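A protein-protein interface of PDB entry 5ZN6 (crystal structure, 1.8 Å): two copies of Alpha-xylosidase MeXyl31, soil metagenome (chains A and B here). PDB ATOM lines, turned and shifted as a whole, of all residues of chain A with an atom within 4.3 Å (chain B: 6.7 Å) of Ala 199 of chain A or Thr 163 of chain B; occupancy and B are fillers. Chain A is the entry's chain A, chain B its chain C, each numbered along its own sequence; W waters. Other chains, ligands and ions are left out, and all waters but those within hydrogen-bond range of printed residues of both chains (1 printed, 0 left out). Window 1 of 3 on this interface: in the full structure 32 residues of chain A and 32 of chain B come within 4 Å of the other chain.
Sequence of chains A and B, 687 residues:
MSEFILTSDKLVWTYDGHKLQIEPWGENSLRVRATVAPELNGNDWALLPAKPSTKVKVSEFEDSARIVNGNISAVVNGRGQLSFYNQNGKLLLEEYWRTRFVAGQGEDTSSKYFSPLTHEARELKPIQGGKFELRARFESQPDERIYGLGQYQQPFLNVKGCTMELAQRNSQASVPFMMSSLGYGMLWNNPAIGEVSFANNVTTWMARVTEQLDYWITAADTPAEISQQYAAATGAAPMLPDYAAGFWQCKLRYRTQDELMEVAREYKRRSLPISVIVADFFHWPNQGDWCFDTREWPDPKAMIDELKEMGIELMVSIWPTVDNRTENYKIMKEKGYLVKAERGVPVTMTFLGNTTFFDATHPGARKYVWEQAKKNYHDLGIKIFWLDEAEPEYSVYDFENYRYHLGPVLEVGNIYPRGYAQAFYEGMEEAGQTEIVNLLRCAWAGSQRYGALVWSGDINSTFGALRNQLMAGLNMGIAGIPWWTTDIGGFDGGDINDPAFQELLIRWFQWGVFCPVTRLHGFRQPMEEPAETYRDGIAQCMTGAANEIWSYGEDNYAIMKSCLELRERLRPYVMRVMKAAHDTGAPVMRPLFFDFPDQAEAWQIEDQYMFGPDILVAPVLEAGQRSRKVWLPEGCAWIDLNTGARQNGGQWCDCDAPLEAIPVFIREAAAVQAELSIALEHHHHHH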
ATOM      1  N   SER A 140     -19.885  14.776 -14.978  1.00  0.00           N
ATOM      2  CA  SER A 140     -21.006  13.852 -15.140  1.00  0.00           C
ATOM      3  C   SER A 140     -21.075  13.459 -16.622  1.00  0.00           C
ATOM      4  O   SER A 140     -20.525  14.164 -17.483  1.00  0.00           O
ATOM      5  CB  SER A 140     -22.306  14.506 -14.683  1.00  0.00           C
ATOM      6  OG  SER A 140     -22.568  15.680 -15.448  1.00  0.00           O
ATOM      7  N   LYS A 160     -27.265   7.564  -9.858  1.00  0.00           N
ATOM      8  CA  LYS A 160     -26.960   8.767 -10.645  1.00  0.00           C
ATOM      9  C   LYS A 160     -28.041   9.785 -10.327  1.00  0.00           C
ATOM     10  O   LYS A 160     -29.230   9.488 -10.446  1.00  0.00           O
ATOM     11  CB  LYS A 160     -26.926   8.469 -12.159  1.00  0.00           C
ATOM     12  CG  LYS A 160     -26.921   9.687 -13.078  1.00  0.00           C
ATOM     13  CD  LYS A 160     -25.691  10.546 -12.885  1.00  0.00           C
ATOM     14  CE  LYS A 160     -25.728  11.762 -13.797  1.00  0.00           C
ATOM     15  NZ  LYS A 160     -25.417  11.439 -15.208  1.00  0.00           N
ATOM     16  N   SER A 197     -21.546  13.030  -4.256  1.00  0.00           N
ATOM     17  CA  SER A 197     -22.713  13.518  -4.995  1.00  0.00           C
ATOM     18  C   SER A 197     -22.528  13.198  -6.465  1.00  0.00           C
ATOM     19  O   SER A 197     -21.607  13.714  -7.112  1.00  0.00           O
ATOM     20  CB  SER A 197     -22.937  15.028  -4.801  1.00  0.00           C
ATOM     21  OG  SER A 197     -21.767  15.753  -5.041  1.00  0.00           O
ATOM     22  N   PHE A 198     -23.401  12.336  -6.982  1.00  0.00           N
ATOM     23  CA  PHE A 198     -23.455  12.041  -8.404  1.00  0.00           C
ATOM     24  C   PHE A 198     -24.515  12.949  -8.999  1.00  0.00           C
ATOM     25  O   PHE A 198     -25.517  12.499  -9.560  1.00  0.00           O
ATOM     26  CB  PHE A 198     -23.779  10.569  -8.642  1.00  0.00           C
ATOM     27  CG  PHE A 198     -22.733   9.643  -8.109  1.00  0.00           C
ATOM     28  CD1 PHE A 198     -21.485   9.585  -8.697  1.00  0.00           C
ATOM     29  CD2 PHE A 198     -22.988   8.845  -7.008  1.00  0.00           C
ATOM     30  CE1 PHE A 198     -20.501   8.729  -8.204  1.00  0.00           C
ATOM     31  CE2 PHE A 198     -22.015   7.991  -6.505  1.00  0.00           C
ATOM     32  CZ  PHE A 198     -20.774   7.932  -7.108  1.00  0.00           C
ATOM     33  N   ALA A 199     -24.273  14.244  -8.886  1.00  0.00           N
ATOM     34  CA  ALA A 199     -25.214  15.222  -9.397  1.00  0.00           C
ATOM     35  C   ALA A 199     -25.181  15.209 -10.929  1.00  0.00           C
ATOM     36  O   ALA A 199     -24.166  14.830 -11.550  1.00  0.00           O
ATOM     37  CB  ALA A 199     -24.899  16.593  -8.840  1.00  0.00           C
ATOM     38  N   ASN A 200     -26.295  15.601 -11.538  1.00  0.00           N
ATOM     39  CA  ASN A 200     -26.411  15.576 -12.982  1.00  0.00           C
ATOM     40  C   ASN A 200     -25.400  16.500 -13.648  1.00  0.00           C
ATOM     41  O   ASN A 200     -24.969  16.223 -14.762  1.00  0.00           O
ATOM     42  CB  ASN A 200     -27.822  15.941 -13.450  1.00  0.00           C
ATOM     43  CG  ASN A 200     -28.832  14.850 -13.183  1.00  0.00           C
ATOM     44  OD1 ASN A 200     -28.485  13.692 -12.909  1.00  0.00           O
ATOM     45  ND2 ASN A 200     -30.102  15.209 -13.285  1.00  0.00           N
ATOM     46  N   ASN A 201     -25.024  17.572 -12.945  1.00  0.00           N
ATOM     47  CA  ASN A 201     -24.102  18.574 -13.477  1.00  0.00           C
ATOM     48  C   ASN A 201     -22.602  18.360 -13.186  1.00  0.00           C
ATOM     49  O   ASN A 201     -21.776  18.968 -13.858  1.00  0.00           O
ATOM     50  CB  ASN A 201     -24.552  19.995 -13.095  1.00  0.00           C
ATOM     51  CG  ASN A 201     -24.774  20.189 -11.600  1.00  0.00           C
ATOM     52  OD1 ASN A 201     -25.076  19.251 -10.853  1.00  0.00           O
ATOM     53  ND2 ASN A 201     -24.654  21.430 -11.162  1.00  0.00           N
ATOM     54  N   VAL A 202     -22.264  17.482 -12.234  1.00  0.00           N
ATOM     55  CA  VAL A 202     -20.874  17.216 -11.800  1.00  0.00           C
ATOM     56  C   VAL A 202     -20.860  16.140 -10.694  1.00  0.00           C
ATOM     57  O   VAL A 202     -21.751  16.107  -9.858  1.00  0.00           O
ATOM     58  CB  VAL A 202     -20.169  18.514 -11.277  1.00  0.00           C
ATOM     59  CG1 VAL A 202     -20.991  19.176 -10.188  1.00  0.00           C
ATOM     60  CG2 VAL A 202     -18.744  18.235 -10.789  1.00  0.00           C
ATOM     61  N   TYR B 152     -26.146  29.547 -14.004  1.00  0.00           N
ATOM     62  CA  TYR B 152     -25.145  28.514 -13.807  1.00  0.00           C
ATOM     63  C   TYR B 152     -24.658  28.001 -15.152  1.00  0.00           C
ATOM     64  O   TYR B 152     -25.432  27.849 -16.097  1.00  0.00           O
ATOM     65  CB  TYR B 152     -25.706  27.387 -12.940  1.00  0.00           C
ATOM     66  CG  TYR B 152     -25.888  27.827 -11.512  1.00  0.00           C
ATOM     67  CD1 TYR B 152     -27.050  28.474 -11.108  1.00  0.00           C
ATOM     68  CD2 TYR B 152     -24.869  27.651 -10.571  1.00  0.00           C
ATOM     69  CE1 TYR B 152     -27.202  28.916  -9.810  1.00  0.00           C
ATOM     70  CE2 TYR B 152     -25.019  28.072  -9.263  1.00  0.00           C
ATOM     71  CZ  TYR B 152     -26.186  28.708  -8.882  1.00  0.00           C
ATOM     72  OH  TYR B 152     -26.347  29.145  -7.579  1.00  0.00           O
ATOM     73  N   GLN B 154     -24.006  25.488 -17.129  1.00  0.00           N
ATOM     74  CA  GLN B 154     -24.339  24.065 -17.249  1.00  0.00           C
ATOM     75  C   GLN B 154     -25.525  23.854 -18.208  1.00  0.00           C
ATOM     76  O   GLN B 154     -26.416  24.706 -18.291  1.00  0.00           O
ATOM     77  CB  GLN B 154     -24.651  23.484 -15.858  1.00  0.00           C
ATOM     78  CG  GLN B 154     -25.864  24.133 -15.181  1.00  0.00           C
ATOM     79  CD  GLN B 154     -26.015  23.763 -13.717  1.00  0.00           C
ATOM     80  OE1 GLN B 154     -25.056  23.321 -13.072  1.00  0.00           O
ATOM     81  NE2 GLN B 154     -27.225  23.943 -13.181  1.00  0.00           N
ATOM     82  N   PHE B 156     -28.497  22.507 -18.432  1.00  0.00           N
ATOM     83  CA  PHE B 156     -29.687  21.974 -17.766  1.00  0.00           C
ATOM     84  C   PHE B 156     -30.645  23.131 -17.554  1.00  0.00           C
ATOM     85  O   PHE B 156     -30.282  24.078 -16.874  1.00  0.00           O
ATOM     86  CB  PHE B 156     -29.319  21.352 -16.415  1.00  0.00           C
ATOM     87  CG  PHE B 156     -28.395  20.179 -16.535  1.00  0.00           C
ATOM     88  CD1 PHE B 156     -28.893  18.928 -16.854  1.00  0.00           C
ATOM     89  CD2 PHE B 156     -27.018  20.337 -16.380  1.00  0.00           C
ATOM     90  CE1 PHE B 156     -28.036  17.836 -17.011  1.00  0.00           C
ATOM     91  CE2 PHE B 156     -26.145  19.248 -16.523  1.00  0.00           C
ATOM     92  CZ  PHE B 156     -26.656  18.003 -16.840  1.00  0.00           C
ATOM     93  N   VAL B 159     -33.364  21.705 -13.379  1.00  0.00           N
ATOM     94  CA  VAL B 159     -32.214  21.428 -12.500  1.00  0.00           C
ATOM     95  C   VAL B 159     -32.473  20.370 -11.412  1.00  0.00           C
ATOM     96  O   VAL B 159     -31.648  20.187 -10.513  1.00  0.00           O
ATOM     97  CB  VAL B 159     -31.608  22.721 -11.899  1.00  0.00           C
ATOM     98  CG1 VAL B 159     -31.082  23.609 -13.013  1.00  0.00           C
ATOM     99  CG2 VAL B 159     -32.605  23.485 -11.023  1.00  0.00           C
ATOM    100  N   GLY B 161     -32.062  17.069  -9.801  1.00  0.00           N
ATOM    101  CA  GLY B 161     -30.902  16.180  -9.880  1.00  0.00           C
ATOM    102  C   GLY B 161     -29.557  16.899  -9.928  1.00  0.00           C
ATOM    103  O   GLY B 161     -28.500  16.231  -9.934  1.00  0.00           O
ATOM    104  N   CYS B 162     -29.586  18.236  -9.985  1.00  0.00           N
ATOM    105  CA  CYS B 162     -28.377  19.046 -10.013  1.00  0.00           C
ATOM    106  C   CYS B 162     -28.153  19.661  -8.656  1.00  0.00           C
ATOM    107  O   CYS B 162     -29.105  19.859  -7.887  1.00  0.00           O
ATOM    108  CB  CYS B 162     -28.466  20.189 -11.040  1.00  0.00           C
ATOM    109  SG  CYS B 162     -28.473  19.684 -12.765  1.00  0.00           S
ATOM    110  N   THR B 163     -26.894  19.976  -8.387  1.00  0.00           N
ATOM    111  CA  THR B 163     -26.503  20.694  -7.188  1.00  0.00           C
ATOM    112  C   THR B 163     -25.822  22.005  -7.567  1.00  0.00           C
ATOM    113  O   THR B 163     -24.886  22.019  -8.360  1.00  0.00           O
ATOM    114  CB  THR B 163     -25.607  19.818  -6.313  1.00  0.00           C
ATOM    115  OG1 THR B 163     -26.368  18.671  -5.885  1.00  0.00           O
ATOM    116  CG2 THR B 163     -25.081  20.603  -5.104  1.00  0.00           C
ATOM    117  N   MET B 164     -26.322  23.107  -7.009  1.00  0.00           N
ATOM    118  CA  MET B 164     -25.837  24.446  -7.337  1.00  0.00           C
ATOM    119  C   MET B 164     -25.158  25.096  -6.143  1.00  0.00           C
ATOM    120  O   MET B 164     -25.703  25.112  -5.033  1.00  0.00           O
ATOM    121  CB  MET B 164     -26.990  25.342  -7.805  1.00  0.00           C
ATOM    122  CG  MET B 164     -27.318  25.197  -9.290  1.00  0.00           C
ATOM    123  SD  MET B 164     -27.870  23.553  -9.773  1.00  0.00           S
ATOM    124  CE  MET B 164     -29.450  23.565  -8.937  1.00  0.00           C
ATOM    125  N   GLU B 165     -23.960  25.632  -6.377  1.00  0.00           N
ATOM    126  CA  GLU B 165     -23.257  26.388  -5.355  1.00  0.00           C
ATOM    127  C   GLU B 165     -23.962  27.735  -5.132  1.00  0.00           C
ATOM    128  O   GLU B 165     -24.236  28.476  -6.079  1.00  0.00           O
ATOM    129  CB  GLU B 165     -21.793  26.604  -5.743  1.00  0.00           C
ATOM    130  CG  GLU B 165     -20.975  27.376  -4.710  1.00  0.00           C
ATOM    131  CD  GLU B 165     -19.626  27.825  -5.254  1.00  0.00           C
ATOM    132  OE1 GLU B 165     -19.543  28.238  -6.432  1.00  0.00           O
ATOM    133  OE2 GLU B 165     -18.640  27.786  -4.490  1.00  0.00           O
ATOM    134  N   GLU B 195     -25.070  26.036  -0.514  1.00  0.00           N
ATOM    135  CA  GLU B 195     -25.379  25.122  -1.592  1.00  0.00           C
ATOM    136  C   GLU B 195     -26.872  24.768  -1.596  1.00  0.00           C
ATOM    137  O   GLU B 195     -27.530  24.769  -0.553  1.00  0.00           O
ATOM    138  CB  GLU B 195     -24.487  23.880  -1.425  1.00  0.00           C
ATOM    139  CG  GLU B 195     -24.856  22.691  -2.261  1.00  0.00           C
ATOM    140  CD  GLU B 195     -23.921  21.528  -2.042  1.00  0.00           C
ATOM    141  OE1 GLU B 195     -22.763  21.629  -2.474  1.00  0.00           O
ATOM    142  OE2 GLU B 195     -24.366  20.503  -1.476  1.00  0.00           O
ATOM    143  N   VAL B 196     -27.407  24.491  -2.785  1.00  0.00           N
ATOM    144  CA  VAL B 196     -28.736  23.884  -2.902  1.00  0.00           C
ATOM    145  C   VAL B 196     -28.567  22.601  -3.722  1.00  0.00           C
ATOM    146  O   VAL B 196     -28.103  22.630  -4.861  1.00  0.00           O
ATOM    147  CB  VAL B 196     -29.832  24.849  -3.439  1.00  0.00           C
ATOM    148  CG1 VAL B 196     -29.531  25.366  -4.836  1.00  0.00           C
ATOM    149  CG2 VAL B 196     -31.200  24.172  -3.404  1.00  0.00           C
ATOM    150  N   SER B 197     -28.952  21.492  -3.104  1.00  0.00           N
ATOM    151  CA  SER B 197     -28.881  20.168  -3.693  1.00  0.00           C
ATOM    152  C   SER B 197     -30.298  19.700  -3.994  1.00  0.00           C
ATOM    153  O   SER B 197     -31.065  19.444  -3.071  1.00  0.00           O
ATOM    154  CB  SER B 197     -28.201  19.207  -2.707  1.00  0.00           C
ATOM    155  OG  SER B 197     -28.258  17.865  -3.162  1.00  0.00           O
ATOM    156  N   PHE B 198     -30.655  19.609  -5.275  1.00  0.00           N
ATOM    157  CA  PHE B 198     -31.922  18.977  -5.675  1.00  0.00           C
ATOM    158  C   PHE B 198     -31.671  17.522  -6.039  1.00  0.00           C
ATOM    159  O   PHE B 198     -31.994  17.083  -7.138  1.00  0.00           O
ATOM    160  CB  PHE B 198     -32.579  19.734  -6.821  1.00  0.00           C
ATOM    161  CG  PHE B 198     -32.979  21.135  -6.451  1.00  0.00           C
ATOM    162  CD1 PHE B 198     -33.955  21.354  -5.498  1.00  0.00           C
ATOM    163  CD2 PHE B 198     -32.351  22.226  -7.024  1.00  0.00           C
ATOM    164  CE1 PHE B 198     -34.336  22.651  -5.155  1.00  0.00           C
ATOM    165  CE2 PHE B 198     -32.705  23.519  -6.670  1.00  0.00           C
ATOM    166  CZ  PHE B 198     -33.694  23.729  -5.735  1.00  0.00           C
ATOM    167  N   ALA B 199     -31.128  16.764  -5.097  1.00  0.00           N
ATOM    168  CA  ALA B 199     -30.756  15.384  -5.371  1.00  0.00           C
ATOM    169  C   ALA B 199     -32.031  14.531  -5.469  1.00  0.00           C
ATOM    170  O   ALA B 199     -33.070  14.879  -4.881  1.00  0.00           O
ATOM    171  CB  ALA B 199     -29.826  14.860  -4.285  1.00  0.00           C
HETATM  172  O   HOH W   1     -31.364  18.162 -14.361  1.00  0.00           O
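ND2 of Asn 201 of chain A lies within hydrogen-bond range of OE1 of Gln 154 of chain B, at 2.7 Å. The backbone NH (N) of Asn 200 of chain A lies within hydrogen-bond range of the backbone carbonyl oxygen (O) of Gly 161 of chain B (2.8 Å). The backbone carbonyl oxygen (O) of Thr 163 of chain B lies within hydrogen-bond range of the side-chain amide nitrogen (ND2) of Asn 201 of chain A (2.9 Å).
O of Cys 162 of chain B sits at hydrogen-bond distance from N of Phe 198 of chain B (3.0 Å). OG of Ser 197 of chain B lies within hydrogen-bond range of OG1 of Thr 163 of chain B (3.4 Å). OG of Ser 140 of chain A is in hydrogen-bond range of O of Asn 200 of chain A, at 2.6 Å. The side-chain sulfur of Met 164 of chain B sits at hydrogen-bond distance from the side-chain amide nitrogen of Gln 154 of chain B (3.5 Å). N of Gly 161 of chain B is in hydrogen-bond range of O of Phe 198 of chain B, 2.7 Å away.
Among the printed residues, pairs that only touch across the chains: Ala 199 of chain A with Gly 161 of chain B, Ala 199 of chain A with Thr 163 of chain B, Asn 200 of chain A with Phe 156 of chain B, Asn 200 of chain A with Cys 162 of chain B, Asn 201 of chain A with Phe 156 of chain B and Asn 201 of chain A with Cys 162 of chain B.
Ser 197 of chain A touches none of the printed residues of chain B. Phe 198 of chain A touches none of the printed residues of chain B. Ala 199 of chain A touches just these residues of chain B: Gly 161 and Thr 163. Of the printed residues of chain B, Asn 200 of chain A touches Phe 156 (3.2 Å), Gly 161 (2.8 Å) and Cys 162 (3.9 Å). Printed residues of chain B within 4 Å of Asn 201 of chain A: Gln 154 (2.7 Å), Phe 156 (3.7 Å), Cys 162 (3.4 Å) and Thr 163 (2.9 Å). Of the printed residues of chain A, Phe 156 of chain B touches Asn 200 (3.2 Å) and Asn 201 (3.7 Å). Printed residues of chain A within 4 Å of Gly 161 of chain B: Ala 199 (3.5 Å) and Asn 200 (2.8 Å). Thr 163 of chain B touches just these residues of chain A: Ala 199 and Asn 201. The nearest residue of chain B that does not touch Ala 199 of chain A is Cys 162 of chain B (4.4 Å).
Of the 8 printed residues of chain A, 3 touch a printed residue of chain B. Hydrophobic or aromatic side chains of chain A within 4 Å of the printed part of chain B: Ala 199. Of the 14 printed residues of chain B, 5 touch a printed residue of chain A. Hydrophobic or aromatic side chains of chain B that line the printed part of chain A: Phe 156. Among the printed residues, 9 pairs touch across the chains.
Positions printed for both chains: 197, 198 and 199. Of the 9 pairs that touch across the chains among the printed residues, none has its exchanged pair printed and touching as well.
Water W1 lies within hydrogen-bond range of the side-chain amide nitrogen (ND2) of Asn 200 of chain A and the side-chain sulfur (SG) of Cys 162 of chain B.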
